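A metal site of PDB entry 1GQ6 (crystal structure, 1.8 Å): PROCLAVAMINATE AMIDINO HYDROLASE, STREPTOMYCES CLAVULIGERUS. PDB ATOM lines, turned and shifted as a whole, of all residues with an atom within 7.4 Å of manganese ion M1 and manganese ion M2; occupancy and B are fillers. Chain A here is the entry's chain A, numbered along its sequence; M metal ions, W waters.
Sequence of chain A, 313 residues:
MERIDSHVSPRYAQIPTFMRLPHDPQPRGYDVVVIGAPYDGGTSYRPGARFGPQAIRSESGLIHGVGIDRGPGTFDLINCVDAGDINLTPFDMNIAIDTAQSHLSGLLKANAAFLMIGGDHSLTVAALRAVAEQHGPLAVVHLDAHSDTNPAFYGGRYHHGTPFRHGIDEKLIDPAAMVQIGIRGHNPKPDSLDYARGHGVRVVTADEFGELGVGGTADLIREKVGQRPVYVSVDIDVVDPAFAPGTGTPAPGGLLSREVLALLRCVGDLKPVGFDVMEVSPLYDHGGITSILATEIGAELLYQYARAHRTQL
Manganese ion M2 is bound by the side-chain carboxylate (OD2) of Asp 237 (2.1 Å). Manganese ion M2 is bound by water W2, 2.2 Å away. Manganese ion M2 is bound by the side-chain carboxylate (OD1) of Asp 144 (2.2 Å). ND1 of His 146 binds manganese ion M2 (2.2 Å). The side-chain carboxylate (OD2) of Asp 235 is bound to manganese ion M2, at 2.3 Å. Manganese ion M2 is bound by the side-chain carboxylate (OD1) of Asp 237.
Manganese ion M1 is bound by the side-chain carboxylate (OD2) of Asp 148, at 2.1 Å. Manganese ion M1 is bound by OD2 of Asp 144, at 2.2 Å. OD2 of Asp 235 is bound to manganese ion M1, at 2.2 Å. Water W1 is bound to manganese ion M1. ND1 of His 121 is bound to manganese ion M1. Water W2 is bound to manganese ion M1 (2.3 Å). Manganese ion M1 has six donor atoms within binding distance.
The backbone carbonyl oxygen (O) of Asp 148 is in hydrogen-bond range of the backbone NH (N) of Phe 164, 3.1 Å away. N of Ala 145 lies close to OD1 of Asp 237, at 3.2 Å. The side-chain carboxylate (OD2) of Asp 237 lies close to the side-chain hydroxyl (OG1) of Thr 249 (3.2 Å). The side-chain carboxylate of Asp 144 sits close to a ring nitrogen (NE2) of His 142 (2.9 Å). The backbone NH of Asp 235 sits at hydrogen-bond distance from the backbone carbonyl oxygen of Leu 143. The backbone NH (N) of His 121 lies within hydrogen-bond range of the side-chain carboxylate (OE2) of Glu 279, at 2.9 Å. The side-chain hydroxyl (OG) of Ser 233 lies within hydrogen-bond range of a ring nitrogen (NE2) of His 121 (2.7 Å).
Four residues have an atom within 4 Å of manganese ion M1: His 121, Asp 144, Asp 148 and Asp 235. Along chain A the residues within 4 Å of manganese ion M1 span positions 121 to 235.
Water W1 bridges OE2 of Glu 279 and O of His 160.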
ATOM      1  N   ASP A 120     -20.179 -30.977 -15.402  1.00  0.00           N
ATOM      2  CA  ASP A 120     -19.372 -29.984 -14.716  1.00  0.00           C
ATOM      3  C   ASP A 120     -17.885 -30.288 -14.769  1.00  0.00           C
ATOM      4  O   ASP A 120     -17.490 -31.415 -15.026  1.00  0.00           O
ATOM      5  CB  ASP A 120     -19.889 -29.703 -13.316  1.00  0.00           C
ATOM      6  CG  ASP A 120     -19.472 -30.733 -12.308  1.00  0.00           C
ATOM      7  OD1 ASP A 120     -18.265 -30.779 -11.942  1.00  0.00           O
ATOM      8  OD2 ASP A 120     -20.325 -31.501 -11.825  1.00  0.00           O
ATOM      9  N   HIS A 121     -17.073 -29.274 -14.532  1.00  0.00           N
ATOM     10  CA  HIS A 121     -15.637 -29.362 -14.739  1.00  0.00           C
ATOM     11  C   HIS A 121     -14.915 -30.360 -13.827  1.00  0.00           C
ATOM     12  O   HIS A 121     -13.798 -30.758 -14.126  1.00  0.00           O
ATOM     13  CB  HIS A 121     -15.020 -27.952 -14.614  1.00  0.00           C
ATOM     14  CG  HIS A 121     -13.998 -27.644 -15.645  1.00  0.00           C
ATOM     15  ND1 HIS A 121     -13.639 -26.349 -15.966  1.00  0.00           N
ATOM     16  CD2 HIS A 121     -13.252 -28.467 -16.427  1.00  0.00           C
ATOM     17  CE1 HIS A 121     -12.732 -26.392 -16.923  1.00  0.00           C
ATOM     18  NE2 HIS A 121     -12.457 -27.657 -17.200  1.00  0.00           N
ATOM     19  N   SER A 122     -15.532 -30.768 -12.730  1.00  0.00           N
ATOM     20  CA  SER A 122     -14.864 -31.748 -11.853  1.00  0.00           C
ATOM     21  C   SER A 122     -14.493 -32.997 -12.596  1.00  0.00           C
ATOM     22  O   SER A 122     -13.530 -33.635 -12.257  1.00  0.00           O
ATOM     23  CB  SER A 122     -15.754 -32.133 -10.680  1.00  0.00           C
ATOM     24  OG  SER A 122     -16.967 -32.751 -11.085  1.00  0.00           O
ATOM     25  N   HIS A 142      -6.064 -24.588 -20.715  1.00  0.00           N
ATOM     26  CA  HIS A 142      -7.292 -24.523 -19.926  1.00  0.00           C
ATOM     27  C   HIS A 142      -7.920 -23.162 -20.165  1.00  0.00           C
ATOM     28  O   HIS A 142      -7.299 -22.148 -19.863  1.00  0.00           O
ATOM     29  CB  HIS A 142      -6.955 -24.743 -18.455  1.00  0.00           C
ATOM     30  CG  HIS A 142      -8.084 -24.504 -17.490  1.00  0.00           C
ATOM     31  ND1 HIS A 142      -7.866 -23.995 -16.224  1.00  0.00           N
ATOM     32  CD2 HIS A 142      -9.411 -24.773 -17.557  1.00  0.00           C
ATOM     33  CE1 HIS A 142      -9.008 -23.900 -15.579  1.00  0.00           C
ATOM     34  NE2 HIS A 142      -9.966 -24.375 -16.357  1.00  0.00           N
ATOM     35  N   LEU A 143      -9.142 -23.138 -20.724  1.00  0.00           N
ATOM     36  CA  LEU A 143      -9.859 -21.875 -20.969  1.00  0.00           C
ATOM     37  C   LEU A 143     -10.981 -21.833 -19.944  1.00  0.00           C
ATOM     38  O   LEU A 143     -11.799 -22.745 -19.872  1.00  0.00           O
ATOM     39  CB  LEU A 143     -10.485 -21.818 -22.358  1.00  0.00           C
ATOM     40  CG  LEU A 143      -9.538 -21.968 -23.558  1.00  0.00           C
ATOM     41  CD1 LEU A 143     -10.278 -21.477 -24.822  1.00  0.00           C
ATOM     42  CD2 LEU A 143      -8.268 -21.288 -23.389  1.00  0.00           C
ATOM     43  N   ASP A 144     -11.038 -20.750 -19.173  1.00  0.00           N
ATOM     44  CA  ASP A 144     -11.952 -20.661 -18.046  1.00  0.00           C
ATOM     45  C   ASP A 144     -11.965 -19.243 -17.471  1.00  0.00           C
ATOM     46  O   ASP A 144     -10.979 -18.525 -17.552  1.00  0.00           O
ATOM     47  CB  ASP A 144     -11.428 -21.595 -16.949  1.00  0.00           C
ATOM     48  CG  ASP A 144     -12.538 -22.167 -16.061  1.00  0.00           C
ATOM     49  OD1 ASP A 144     -13.383 -21.412 -15.581  1.00  0.00           O
ATOM     50  OD2 ASP A 144     -12.619 -23.362 -15.777  1.00  0.00           O
ATOM     51  N   ALA A 145     -13.091 -18.835 -16.869  1.00  0.00           N
ATOM     52  CA  ALA A 145     -13.106 -17.597 -16.110  1.00  0.00           C
ATOM     53  C   ALA A 145     -12.518 -17.800 -14.737  1.00  0.00           C
ATOM     54  O   ALA A 145     -12.231 -16.813 -14.043  1.00  0.00           O
ATOM     55  CB  ALA A 145     -14.520 -17.123 -15.927  1.00  0.00           C
ATOM     56  N   HIS A 146     -12.369 -19.068 -14.343  1.00  0.00           N
ATOM     57  CA  HIS A 146     -11.911 -19.427 -12.984  1.00  0.00           C
ATOM     58  C   HIS A 146     -10.740 -20.394 -13.078  1.00  0.00           C
ATOM     59  O   HIS A 146     -10.679 -21.216 -13.969  1.00  0.00           O
ATOM     60  CB  HIS A 146     -13.059 -20.119 -12.254  1.00  0.00           C
ATOM     61  CG  HIS A 146     -14.364 -19.430 -12.413  1.00  0.00           C
ATOM     62  ND1 HIS A 146     -15.251 -19.764 -13.408  1.00  0.00           N
ATOM     63  CD2 HIS A 146     -14.902 -18.393 -11.742  1.00  0.00           C
ATOM     64  CE1 HIS A 146     -16.310 -18.970 -13.322  1.00  0.00           C
ATOM     65  NE2 HIS A 146     -16.114 -18.127 -12.330  1.00  0.00           N
ATOM     66  N   SER A 147      -9.819 -20.312 -12.117  1.00  0.00           N
ATOM     67  CA  SER A 147      -8.604 -21.121 -12.137  1.00  0.00           C
ATOM     68  C   SER A 147      -8.850 -22.607 -11.875  1.00  0.00           C
ATOM     69  O   SER A 147      -8.132 -23.446 -12.399  1.00  0.00           O
ATOM     70  CB  SER A 147      -7.609 -20.586 -11.129  1.00  0.00           C
ATOM     71  OG  SER A 147      -6.434 -21.346 -11.146  1.00  0.00           O
ATOM     72  N   ASP A 148      -9.848 -22.922 -11.055  1.00  0.00           N
ATOM     73  CA  ASP A 148     -10.199 -24.308 -10.750  1.00  0.00           C
ATOM     74  C   ASP A 148      -8.999 -25.085 -10.158  1.00  0.00           C
ATOM     75  O   ASP A 148      -8.791 -26.284 -10.443  1.00  0.00           O
ATOM     76  CB  ASP A 148     -10.766 -25.050 -11.955  1.00  0.00           C
ATOM     77  CG  ASP A 148     -12.130 -24.540 -12.396  1.00  0.00           C
ATOM     78  OD1 ASP A 148     -12.724 -23.642 -11.753  1.00  0.00           O
ATOM     79  OD2 ASP A 148     -12.684 -25.016 -13.357  1.00  0.00           O
ATOM     80  N   HIS A 160     -16.318 -28.653  -8.393  1.00  0.00           N
ATOM     81  CA  HIS A 160     -15.852 -28.243  -9.708  1.00  0.00           C
ATOM     82  C   HIS A 160     -14.762 -27.205  -9.736  1.00  0.00           C
ATOM     83  O   HIS A 160     -14.333 -26.816 -10.792  1.00  0.00           O
ATOM     84  CB  HIS A 160     -17.019 -27.857 -10.612  1.00  0.00           C
ATOM     85  CG  HIS A 160     -17.763 -26.638 -10.179  1.00  0.00           C
ATOM     86  ND1 HIS A 160     -18.547 -25.913 -11.066  1.00  0.00           N
ATOM     87  CD2 HIS A 160     -17.877 -26.024  -8.987  1.00  0.00           C
ATOM     88  CE1 HIS A 160     -19.117 -24.917 -10.409  1.00  0.00           C
ATOM     89  NE2 HIS A 160     -18.715 -24.956  -9.144  1.00  0.00           N
ATOM     90  N   GLY A 161     -14.319 -26.773  -8.574  1.00  0.00           N
ATOM     91  CA  GLY A 161     -13.204 -25.856  -8.480  1.00  0.00           C
ATOM     92  C   GLY A 161     -11.891 -26.551  -8.200  1.00  0.00           C
ATOM     93  O   GLY A 161     -10.863 -25.871  -7.990  1.00  0.00           O
ATOM     94  N   PRO A 163     -10.439 -29.496 -10.288  1.00  0.00           N
ATOM     95  CA  PRO A 163      -9.799 -30.465 -11.194  1.00  0.00           C
ATOM     96  C   PRO A 163      -8.342 -30.230 -11.473  1.00  0.00           C
ATOM     97  O   PRO A 163      -7.536 -31.204 -11.526  1.00  0.00           O
ATOM     98  CB  PRO A 163     -10.620 -30.352 -12.491  1.00  0.00           C
ATOM     99  CG  PRO A 163     -11.319 -29.061 -12.357  1.00  0.00           C
ATOM    100  CD  PRO A 163     -11.627 -28.878 -10.904  1.00  0.00           C
ATOM    101  N   PHE A 164      -7.936 -28.972 -11.639  1.00  0.00           N
ATOM    102  CA  PHE A 164      -6.524 -28.746 -11.921  1.00  0.00           C
ATOM    103  C   PHE A 164      -5.607 -28.805 -10.701  1.00  0.00           C
ATOM    104  O   PHE A 164      -4.427 -28.987 -10.852  1.00  0.00           O
ATOM    105  CB  PHE A 164      -6.353 -27.500 -12.797  1.00  0.00           C
ATOM    106  CG  PHE A 164      -7.156 -27.616 -14.060  1.00  0.00           C
ATOM    107  CD1 PHE A 164      -6.665 -28.296 -15.144  1.00  0.00           C
ATOM    108  CD2 PHE A 164      -8.439 -27.140 -14.106  1.00  0.00           C
ATOM    109  CE1 PHE A 164      -7.439 -28.489 -16.260  1.00  0.00           C
ATOM    110  CE2 PHE A 164      -9.225 -27.351 -15.230  1.00  0.00           C
ATOM    111  CZ  PHE A 164      -8.706 -28.001 -16.307  1.00  0.00           C
ATOM    112  N   SER A 233      -8.842 -28.198 -22.213  1.00  0.00           N
ATOM    113  CA  SER A 233     -10.069 -28.215 -21.425  1.00  0.00           C
ATOM    114  C   SER A 233     -10.736 -26.859 -21.452  1.00  0.00           C
ATOM    115  O   SER A 233     -10.147 -25.863 -21.041  1.00  0.00           O
ATOM    116  CB  SER A 233      -9.737 -28.623 -19.992  1.00  0.00           C
ATOM    117  OG  SER A 233     -10.916 -28.714 -19.188  1.00  0.00           O
ATOM    118  N   VAL A 234     -11.942 -26.807 -21.997  1.00  0.00           N
ATOM    119  CA  VAL A 234     -12.657 -25.555 -22.121  1.00  0.00           C
ATOM    120  C   VAL A 234     -13.872 -25.549 -21.204  1.00  0.00           C
ATOM    121  O   VAL A 234     -14.767 -26.374 -21.343  1.00  0.00           O
ATOM    122  CB  VAL A 234     -13.153 -25.312 -23.565  1.00  0.00           C
ATOM    123  CG1 VAL A 234     -13.827 -23.970 -23.700  1.00  0.00           C
ATOM    124  CG2 VAL A 234     -12.018 -25.446 -24.528  1.00  0.00           C
ATOM    125  N   ASP A 235     -13.893 -24.583 -20.283  1.00  0.00           N
ATOM    126  CA  ASP A 235     -15.087 -24.273 -19.490  1.00  0.00           C
ATOM    127  C   ASP A 235     -15.825 -23.219 -20.331  1.00  0.00           C
ATOM    128  O   ASP A 235     -15.281 -22.171 -20.646  1.00  0.00           O
ATOM    129  CB  ASP A 235     -14.679 -23.676 -18.130  1.00  0.00           C
ATOM    130  CG  ASP A 235     -15.850 -23.450 -17.176  1.00  0.00           C
ATOM    131  OD1 ASP A 235     -16.969 -23.182 -17.625  1.00  0.00           O
ATOM    132  OD2 ASP A 235     -15.682 -23.455 -15.924  1.00  0.00           O
ATOM    133  N   ILE A 236     -17.060 -23.506 -20.696  1.00  0.00           N
ATOM    134  CA  ILE A 236     -17.849 -22.595 -21.523  1.00  0.00           C
ATOM    135  C   ILE A 236     -17.966 -21.206 -20.888  1.00  0.00           C
ATOM    136  O   ILE A 236     -18.150 -20.214 -21.618  1.00  0.00           O
ATOM    137  CB  ILE A 236     -19.222 -23.219 -21.846  1.00  0.00           C
ATOM    138  CG1 ILE A 236     -19.812 -22.612 -23.138  1.00  0.00           C
ATOM    139  CG2 ILE A 236     -20.209 -23.068 -20.677  1.00  0.00           C
ATOM    140  CD1 ILE A 236     -19.066 -22.961 -24.370  1.00  0.00           C
ATOM    141  N   ASP A 237     -17.781 -21.117 -19.571  1.00  0.00           N
ATOM    142  CA  ASP A 237     -17.894 -19.825 -18.889  1.00  0.00           C
ATOM    143  C   ASP A 237     -16.697 -18.899 -19.139  1.00  0.00           C
ATOM    144  O   ASP A 237     -16.674 -17.770 -18.672  1.00  0.00           O
ATOM    145  CB  ASP A 237     -18.248 -19.997 -17.392  1.00  0.00           C
ATOM    146  CG  ASP A 237     -17.129 -20.484 -16.499  1.00  0.00           C
ATOM    147  OD1 ASP A 237     -15.932 -20.378 -16.854  1.00  0.00           O
ATOM    148  OD2 ASP A 237     -17.427 -20.968 -15.352  1.00  0.00           O
ATOM    149  N   VAL A 238     -15.749 -19.335 -19.966  1.00  0.00           N
ATOM    150  CA  VAL A 238     -14.658 -18.476 -20.360  1.00  0.00           C
ATOM    151  C   VAL A 238     -15.180 -17.294 -21.206  1.00  0.00           C
ATOM    152  O   VAL A 238     -14.631 -16.168 -21.129  1.00  0.00           O
ATOM    153  CB  VAL A 238     -13.538 -19.236 -21.115  1.00  0.00           C
ATOM    154  CG1 VAL A 238     -14.049 -19.736 -22.454  1.00  0.00           C
ATOM    155  CG2 VAL A 238     -12.299 -18.327 -21.286  1.00  0.00           C
ATOM    156  N   THR A 247     -24.818 -21.477 -18.191  1.00  0.00           N
ATOM    157  CA  THR A 247     -23.706 -22.025 -17.439  1.00  0.00           C
ATOM    158  C   THR A 247     -23.929 -21.754 -15.952  1.00  0.00           C
ATOM    159  O   THR A 247     -24.701 -20.856 -15.589  1.00  0.00           O
ATOM    160  CB  THR A 247     -22.371 -21.507 -17.957  1.00  0.00           C
ATOM    161  OG1 THR A 247     -21.299 -22.303 -17.424  1.00  0.00           O
ATOM    162  CG2 THR A 247     -22.080 -20.075 -17.529  1.00  0.00           C
ATOM    163  N   THR A 249     -21.753 -20.881 -13.246  1.00  0.00           N
ATOM    164  CA  THR A 249     -21.128 -19.789 -12.551  1.00  0.00           C
ATOM    165  C   THR A 249     -20.661 -18.774 -13.568  1.00  0.00           C
ATOM    166  O   THR A 249     -19.457 -18.671 -13.831  1.00  0.00           O
ATOM    167  CB  THR A 249     -19.927 -20.253 -11.722  1.00  0.00           C
ATOM    168  OG1 THR A 249     -19.026 -21.030 -12.540  1.00  0.00           O
ATOM    169  CG2 THR A 249     -20.387 -21.172 -10.548  1.00  0.00           C
ATOM    170  N   PRO A 250     -21.592 -17.993 -14.104  1.00  0.00           N
ATOM    171  CA  PRO A 250     -21.207 -16.970 -15.075  1.00  0.00           C
ATOM    172  C   PRO A 250     -20.347 -15.917 -14.439  1.00  0.00           C
ATOM    173  O   PRO A 250     -20.470 -15.658 -13.251  1.00  0.00           O
ATOM    174  CB  PRO A 250     -22.523 -16.326 -15.488  1.00  0.00           C
ATOM    175  CG  PRO A 250     -23.625 -17.246 -14.962  1.00  0.00           C
ATOM    176  CD  PRO A 250     -23.043 -18.028 -13.843  1.00  0.00           C
ATOM    177  N   ALA A 251     -19.496 -15.307 -15.266  1.00  0.00           N
ATOM    178  CA  ALA A 251     -18.586 -14.278 -14.831  1.00  0.00           C
ATOM    179  C   ALA A 251     -18.562 -13.143 -15.843  1.00  0.00           C
ATOM    180  O   ALA A 251     -17.964 -13.301 -16.919  1.00  0.00           O
ATOM    181  CB  ALA A 251     -17.182 -14.866 -14.637  1.00  0.00           C
ATOM    182  N   MET A 278     -16.909 -28.200 -21.083  1.00  0.00           N
ATOM    183  CA  MET A 278     -17.619 -28.390 -19.848  1.00  0.00           C
ATOM    184  C   MET A 278     -18.486 -27.211 -19.433  1.00  0.00           C
ATOM    185  O   MET A 278     -18.320 -26.084 -19.927  1.00  0.00           O
ATOM    186  CB  MET A 278     -16.583 -28.668 -18.755  1.00  0.00           C
ATOM    187  CG  MET A 278     -15.522 -29.719 -19.123  1.00  0.00           C
ATOM    188  SD  MET A 278     -16.218 -31.271 -19.609  1.00  0.00           S
ATOM    189  CE  MET A 278     -16.478 -32.053 -18.015  1.00  0.00           C
ATOM    190  N   GLU A 279     -19.379 -27.508 -18.502  1.00  0.00           N
ATOM    191  CA  GLU A 279     -20.196 -26.551 -17.756  1.00  0.00           C
ATOM    192  C   GLU A 279     -21.373 -25.954 -18.503  1.00  0.00           C
ATOM    193  O   GLU A 279     -21.978 -24.986 -18.045  1.00  0.00           O
ATOM    194  CB  GLU A 279     -19.381 -25.455 -17.054  1.00  0.00           C
ATOM    195  CG  GLU A 279     -18.388 -25.986 -16.015  1.00  0.00           C
ATOM    196  CD  GLU A 279     -18.982 -26.297 -14.654  1.00  0.00           C
ATOM    197  OE1 GLU A 279     -20.204 -26.222 -14.494  1.00  0.00           O
ATOM    198  OE2 GLU A 279     -18.213 -26.685 -13.777  1.00  0.00           O
HETATM  199 MN    MN M   1     -14.148 -24.539 -14.747  1.00  0.00          MN
HETATM  200 MN    MN M   2     -15.424 -21.472 -14.855  1.00  0.00          MN
HETATM  201  O   HOH W   1     -15.638 -25.345 -13.288  1.00  0.00           O
HETATM  202  O   HOH W   2     -14.891 -22.858 -13.293  1.00  0.00           O
